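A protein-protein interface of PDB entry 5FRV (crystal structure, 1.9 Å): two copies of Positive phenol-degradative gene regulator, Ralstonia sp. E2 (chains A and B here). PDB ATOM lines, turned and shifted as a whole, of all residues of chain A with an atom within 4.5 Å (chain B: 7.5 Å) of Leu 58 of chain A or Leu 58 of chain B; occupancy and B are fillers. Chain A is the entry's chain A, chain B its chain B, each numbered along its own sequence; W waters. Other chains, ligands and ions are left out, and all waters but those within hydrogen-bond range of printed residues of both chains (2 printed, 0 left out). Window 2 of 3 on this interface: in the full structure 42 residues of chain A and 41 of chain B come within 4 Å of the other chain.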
ATOM      1  N   LEU A  54      -2.786   3.778  24.003  1.00  0.00           N
ATOM      2  CA  LEU A  54      -2.141   3.874  25.309  1.00  0.00           C
ATOM      3  C   LEU A  54      -2.336   2.594  26.126  1.00  0.00           C
ATOM      4  O   LEU A  54      -1.419   2.144  26.813  1.00  0.00           O
ATOM      5  CB  LEU A  54      -2.672   5.082  26.090  1.00  0.00           C
ATOM      6  CG  LEU A  54      -2.306   6.448  25.516  1.00  0.00           C
ATOM      7  CD1 LEU A  54      -2.814   7.570  26.396  1.00  0.00           C
ATOM      8  CD2 LEU A  54      -0.806   6.552  25.336  1.00  0.00           C
ATOM      9  N   VAL A  55      -3.530   2.018  26.057  1.00  0.00           N
ATOM     10  CA  VAL A  55      -3.823   0.801  26.806  1.00  0.00           C
ATOM     11  C   VAL A  55      -3.020  -0.362  26.239  1.00  0.00           C
ATOM     12  O   VAL A  55      -2.449  -1.159  26.982  1.00  0.00           O
ATOM     13  CB  VAL A  55      -5.332   0.454  26.783  1.00  0.00           C
ATOM     14  CG1 VAL A  55      -5.580  -0.973  27.283  1.00  0.00           C
ATOM     15  CG2 VAL A  55      -6.137   1.467  27.592  1.00  0.00           C
ATOM     16  N   ASP A  56      -2.953  -0.432  24.915  1.00  0.00           N
ATOM     17  CA  ASP A  56      -2.300  -1.552  24.246  1.00  0.00           C
ATOM     18  C   ASP A  56      -0.788  -1.503  24.413  1.00  0.00           C
ATOM     19  O   ASP A  56      -0.139  -2.543  24.493  1.00  0.00           O
ATOM     20  CB  ASP A  56      -2.679  -1.597  22.753  1.00  0.00           C
ATOM     21  CG  ASP A  56      -4.120  -2.047  22.533  1.00  0.00           C
ATOM     22  OD1 ASP A  56      -4.702  -2.672  23.456  1.00  0.00           O
ATOM     23  OD2 ASP A  56      -4.674  -1.786  21.441  1.00  0.00           O
ATOM     24  N   THR A  57      -0.212  -0.308  24.483  1.00  0.00           N
ATOM     25  CA  THR A  57       1.240  -0.218  24.587  1.00  0.00           C
ATOM     26  C   THR A  57       1.739  -0.031  26.023  1.00  0.00           C
ATOM     27  O   THR A  57       2.805  -0.536  26.377  1.00  0.00           O
ATOM     28  CB  THR A  57       1.792   0.931  23.721  1.00  0.00           C
ATOM     29  OG1 THR A  57       1.182   2.164  24.117  1.00  0.00           O
ATOM     30  CG2 THR A  57       1.498   0.676  22.255  1.00  0.00           C
ATOM     31  N   LEU A  58       0.983   0.687  26.851  1.00  0.00           N
ATOM     32  CA  LEU A  58       1.440   0.992  28.210  1.00  0.00           C
ATOM     33  C   LEU A  58       0.796   0.139  29.293  1.00  0.00           C
ATOM     34  O   LEU A  58       1.259   0.139  30.427  1.00  0.00           O
ATOM     35  CB  LEU A  58       1.178   2.451  28.555  1.00  0.00           C
ATOM     36  CG  LEU A  58       1.565   3.519  27.546  1.00  0.00           C
ATOM     37  CD1 LEU A  58       1.250   4.878  28.141  1.00  0.00           C
ATOM     38  CD2 LEU A  58       3.030   3.398  27.173  1.00  0.00           C
ATOM     39  N   GLY A  59      -0.284  -0.553  28.954  1.00  0.00           N
ATOM     40  CA  GLY A  59      -1.030  -1.312  29.937  1.00  0.00           C
ATOM     41  C   GLY A  59      -2.231  -0.528  30.416  1.00  0.00           C
ATOM     42  O   GLY A  59      -2.221   0.700  30.392  1.00  0.00           O
ATOM     43  N   ARG A  62      -1.618   1.975  33.663  1.00  0.00           N
ATOM     44  CA  ARG A  62      -0.799   3.154  33.413  1.00  0.00           C
ATOM     45  C   ARG A  62      -1.565   4.148  32.518  1.00  0.00           C
ATOM     46  O   ARG A  62      -1.428   5.366  32.677  1.00  0.00           O
ATOM     47  CB  ARG A  62       0.535   2.739  32.791  1.00  0.00           C
ATOM     48  CG  ARG A  62       1.309   3.863  32.112  1.00  0.00           C
ATOM     49  CD  ARG A  62       2.175   4.644  33.104  1.00  0.00           C
ATOM     50  NE  ARG A  62       2.873   5.748  32.445  1.00  0.00           N
ATOM     51  CZ  ARG A  62       3.227   6.884  33.042  1.00  0.00           C
ATOM     52  NH1 ARG A  62       2.952   7.091  34.323  1.00  0.00           N
ATOM     53  NH2 ARG A  62       3.848   7.823  32.346  1.00  0.00           N
ATOM     54  N   LEU A  66      -2.946   8.161  33.306  1.00  0.00           N
ATOM     55  CA  LEU A  66      -2.821   9.330  32.426  1.00  0.00           C
ATOM     56  C   LEU A  66      -4.164  10.052  32.242  1.00  0.00           C
ATOM     57  O   LEU A  66      -4.222  11.286  32.297  1.00  0.00           O
ATOM     58  CB  LEU A  66      -2.240   8.932  31.056  1.00  0.00           C
ATOM     59  CG  LEU A  66      -0.784   8.437  30.973  1.00  0.00           C
ATOM     60  CD1 LEU A  66      -0.561   7.678  29.674  1.00  0.00           C
ATOM     61  CD2 LEU A  66       0.182   9.577  31.071  1.00  0.00           C
ATOM     62  N   LYS B  52       2.823  16.619  27.920  1.00  0.00           N
ATOM     63  CA  LYS B  52       4.060  16.653  28.681  1.00  0.00           C
ATOM     64  C   LYS B  52       4.359  15.275  29.271  1.00  0.00           C
ATOM     65  O   LYS B  52       5.495  14.801  29.205  1.00  0.00           O
ATOM     66  CB  LYS B  52       4.001  17.704  29.788  1.00  0.00           C
ATOM     67  CG  LYS B  52       5.214  17.625  30.707  1.00  0.00           C
ATOM     68  CD  LYS B  52       5.439  18.894  31.485  1.00  0.00           C
ATOM     69  CE  LYS B  52       6.798  18.834  32.181  1.00  0.00           C
ATOM     70  NZ  LYS B  52       7.907  18.757  31.177  1.00  0.00           N
ATOM     71  N   GLU B  53       3.338  14.625  29.827  1.00  0.00           N
ATOM     72  CA  GLU B  53       3.518  13.300  30.406  1.00  0.00           C
ATOM     73  C   GLU B  53       3.994  12.286  29.378  1.00  0.00           C
ATOM     74  O   GLU B  53       4.875  11.473  29.680  1.00  0.00           O
ATOM     75  CB  GLU B  53       2.228  12.809  31.058  1.00  0.00           C
ATOM     76  CG  GLU B  53       1.985  13.395  32.445  1.00  0.00           C
ATOM     77  CD  GLU B  53       1.101  12.519  33.295  1.00  0.00           C
ATOM     78  OE1 GLU B  53       1.497  11.363  33.568  1.00  0.00           O
ATOM     79  OE2 GLU B  53       0.002  12.980  33.679  1.00  0.00           O
ATOM     80  N   LEU B  54       3.398  12.319  28.182  1.00  0.00           N
ATOM     81  CA  LEU B  54       3.759  11.416  27.095  1.00  0.00           C
ATOM     82  C   LEU B  54       5.182  11.653  26.613  1.00  0.00           C
ATOM     83  O   LEU B  54       5.931  10.699  26.403  1.00  0.00           O
ATOM     84  CB  LEU B  54       2.779  11.564  25.911  1.00  0.00           C
ATOM     85  CG  LEU B  54       1.385  11.007  26.221  1.00  0.00           C
ATOM     86  CD1 LEU B  54       0.429  11.036  25.022  1.00  0.00           C
ATOM     87  CD2 LEU B  54       1.507   9.591  26.782  1.00  0.00           C
ATOM     88  N   VAL B  55       5.537  12.917  26.405  1.00  0.00           N
ATOM     89  CA  VAL B  55       6.871  13.278  25.928  1.00  0.00           C
ATOM     90  C   VAL B  55       7.955  12.894  26.940  1.00  0.00           C
ATOM     91  O   VAL B  55       9.038  12.432  26.561  1.00  0.00           O
ATOM     92  CB  VAL B  55       6.972  14.794  25.618  1.00  0.00           C
ATOM     93  CG1 VAL B  55       8.424  15.235  25.541  1.00  0.00           C
ATOM     94  CG2 VAL B  55       6.251  15.116  24.299  1.00  0.00           C
ATOM     95  N   ASP B  56       7.649  13.074  28.223  1.00  0.00           N
ATOM     96  CA  ASP B  56       8.611  12.786  29.283  1.00  0.00           C
ATOM     97  C   ASP B  56       8.844  11.282  29.437  1.00  0.00           C
ATOM     98  O   ASP B  56       9.949  10.855  29.747  1.00  0.00           O
ATOM     99  CB  ASP B  56       8.141  13.376  30.620  1.00  0.00           C
ATOM    100  CG  ASP B  56       8.311  14.895  30.694  1.00  0.00           C
ATOM    101  OD1 ASP B  56       8.930  15.489  29.783  1.00  0.00           O
ATOM    102  OD2 ASP B  56       7.825  15.499  31.681  1.00  0.00           O
ATOM    103  N   THR B  57       7.805  10.484  29.223  1.00  0.00           N
ATOM    104  CA  THR B  57       7.880   9.056  29.505  1.00  0.00           C
ATOM    105  C   THR B  57       8.061   8.175  28.273  1.00  0.00           C
ATOM    106  O   THR B  57       8.595   7.075  28.375  1.00  0.00           O
ATOM    107  CB  THR B  57       6.629   8.584  30.241  1.00  0.00           C
ATOM    108  OG1 THR B  57       5.485   8.830  29.420  1.00  0.00           O
ATOM    109  CG2 THR B  57       6.483   9.331  31.562  1.00  0.00           C
ATOM    110  N   LEU B  58       7.599   8.636  27.115  1.00  0.00           N
ATOM    111  CA  LEU B  58       7.700   7.830  25.903  1.00  0.00           C
ATOM    112  C   LEU B  58       8.692   8.432  24.922  1.00  0.00           C
ATOM    113  O   LEU B  58       9.140   7.761  24.001  1.00  0.00           O
ATOM    114  CB  LEU B  58       6.341   7.678  25.226  1.00  0.00           C
ATOM    115  CG  LEU B  58       5.232   7.008  26.036  1.00  0.00           C
ATOM    116  CD1 LEU B  58       4.092   6.581  25.109  1.00  0.00           C
ATOM    117  CD2 LEU B  58       5.767   5.826  26.819  1.00  0.00           C
ATOM    118  N   GLY B  59       9.021   9.701  25.120  1.00  0.00           N
ATOM    119  CA  GLY B  59       9.916  10.400  24.221  1.00  0.00           C
ATOM    120  C   GLY B  59       9.187  11.235  23.178  1.00  0.00           C
ATOM    121  O   GLY B  59       8.027  10.974  22.853  1.00  0.00           O
ATOM    122  N   MET B  60       9.887  12.233  22.648  1.00  0.00           N
ATOM    123  CA  MET B  60       9.308  13.200  21.725  1.00  0.00           C
ATOM    124  C   MET B  60       8.714  12.522  20.493  1.00  0.00           C
ATOM    125  O   MET B  60       7.580  12.801  20.114  1.00  0.00           O
ATOM    126  CB  MET B  60      10.364  14.230  21.308  1.00  0.00           C
ATOM    127  CG  MET B  60       9.807  15.520  20.691  1.00  0.00           C
ATOM    128  SD  MET B  60       9.049  16.683  21.865  1.00  0.00           S
ATOM    129  CE  MET B  60      10.433  17.095  22.934  1.00  0.00           C
ATOM    130  N   GLU B  61       9.462  11.604  19.891  1.00  0.00           N
ATOM    131  CA  GLU B  61       9.049  11.028  18.610  1.00  0.00           C
ATOM    132  C   GLU B  61       7.910  10.024  18.726  1.00  0.00           C
ATOM    133  O   GLU B  61       7.136   9.871  17.787  1.00  0.00           O
ATOM    134  CB  GLU B  61      10.244  10.383  17.907  1.00  0.00           C
ATOM    135  CG  GLU B  61      10.846  11.285  16.826  1.00  0.00           C
ATOM    136  CD  GLU B  61      12.052  10.672  16.136  1.00  0.00           C
ATOM    137  OE1 GLU B  61      12.224   9.434  16.218  1.00  0.00           O
ATOM    138  OE2 GLU B  61      12.827  11.434  15.507  1.00  0.00           O
ATOM    139  N   ARG B  62       7.786   9.347  19.860  1.00  0.00           N
ATOM    140  CA  ARG B  62       6.646   8.455  20.066  1.00  0.00           C
ATOM    141  C   ARG B  62       5.393   9.262  20.388  1.00  0.00           C
ATOM    142  O   ARG B  62       4.302   8.931  19.936  1.00  0.00           O
ATOM    143  CB  ARG B  62       6.928   7.453  21.189  1.00  0.00           C
ATOM    144  CG  ARG B  62       7.399   6.097  20.704  1.00  0.00           C
ATOM    145  CD  ARG B  62       6.252   5.317  20.074  1.00  0.00           C
ATOM    146  NE  ARG B  62       5.266   4.917  21.077  1.00  0.00           N
ATOM    147  CZ  ARG B  62       3.955   4.857  20.860  1.00  0.00           C
ATOM    148  NH1 ARG B  62       3.461   5.175  19.667  1.00  0.00           N
ATOM    149  NH2 ARG B  62       3.139   4.481  21.837  1.00  0.00           N
ATOM    150  N   ALA B  63       5.559  10.314  21.187  1.00  0.00           N
ATOM    151  CA  ALA B  63       4.459  11.208  21.538  1.00  0.00           C
ATOM    152  C   ALA B  63       3.954  11.952  20.305  1.00  0.00           C
ATOM    153  O   ALA B  63       2.759  12.182  20.152  1.00  0.00           O
ATOM    154  CB  ALA B  63       4.895  12.201  22.607  1.00  0.00           C
ATOM    155  N   LEU B  66       1.683   9.500  18.389  1.00  0.00           N
ATOM    156  CA  LEU B  66       0.406   9.322  19.090  1.00  0.00           C
ATOM    157  C   LEU B  66      -0.555  10.469  18.748  1.00  0.00           C
ATOM    158  O   LEU B  66      -1.717  10.236  18.443  1.00  0.00           O
ATOM    159  CB  LEU B  66       0.612   9.252  20.610  1.00  0.00           C
ATOM    160  CG  LEU B  66       1.306   8.005  21.147  1.00  0.00           C
ATOM    161  CD1 LEU B  66       1.665   8.179  22.621  1.00  0.00           C
ATOM    162  CD2 LEU B  66       0.416   6.797  20.928  1.00  0.00           C
HETATM  163  O   HOH W   1       4.183  10.225  33.819  1.00  0.00           O
HETATM  164  O   HOH W   2      -2.225  13.193  31.985  1.00  0.00           O
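The backbone carbonyl oxygen of Glu 53 of chain B sits at hydrogen-bond distance from the side-chain hydroxyl of Thr 57 of chain B, at 2.7 Å.
Among the printed residues, merely in contact across the chains: Thr 57 of chain A with Arg 62 of chain B (3.8 Å), Leu 58 of chain A with Leu 58 of chain B (3.7 Å) and Leu 66 of chain A with Glu 53 of chain B (3.3 Å).
Of the 13 printed residues of chain B, 4 touch a printed residue of chain A. Hydrophobic or aromatic side chains of chain B that line the printed part of chain A: Leu 58. Hydrophobic or aromatic side chains of chain A that line the printed part of chain B: Leu 58 and Leu 66. Among the printed residues, 4 pairs touch across the chains.
The guanidinium group (NH2) of Arg 62 of chain A sits close to the side-chain hydroxyl (OG1) of Thr 57 of chain B (3.5 Å).
Printed residues of chain B within 4 Å of Leu 58 of chain A: Leu 58 (3.7 Å). Leu 58 of chain B touches just one residue of chain A: Leu 58. Gly 59 of chain A touches none of the printed residues of chain B. Of the printed residues of chain B, Leu 66 of chain A touches Glu 53 (3.3 Å). Of the printed residues of chain A, Arg 62 of chain B touches Thr 57. Ala 63 of chain B touches none of the printed residues of chain A. The nearest printed residue of chain A that does not touch Leu 58 of chain B is Leu 54 of chain A (4.9 Å).
Water W2 bridges O of Leu 66 of chain A (2.8 Å) and OE2 of Glu 53 of chain B (2.8 Å). Water W1 bridges NH2 of Arg 62 of chain A and OE1 of Glu 53 of chain B.
Thr 57 of chain A touches Arg 62 of chain B, and with the chains exchanged Arg 62 of chain A touches Thr 57 of chain B. Leu 58 of chain A touches its own counterpart, Leu 58 of chain B. Of the 4 pairs that touch across the chains among the printed residues, 3 have their exchanged pair printed and touching as well.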
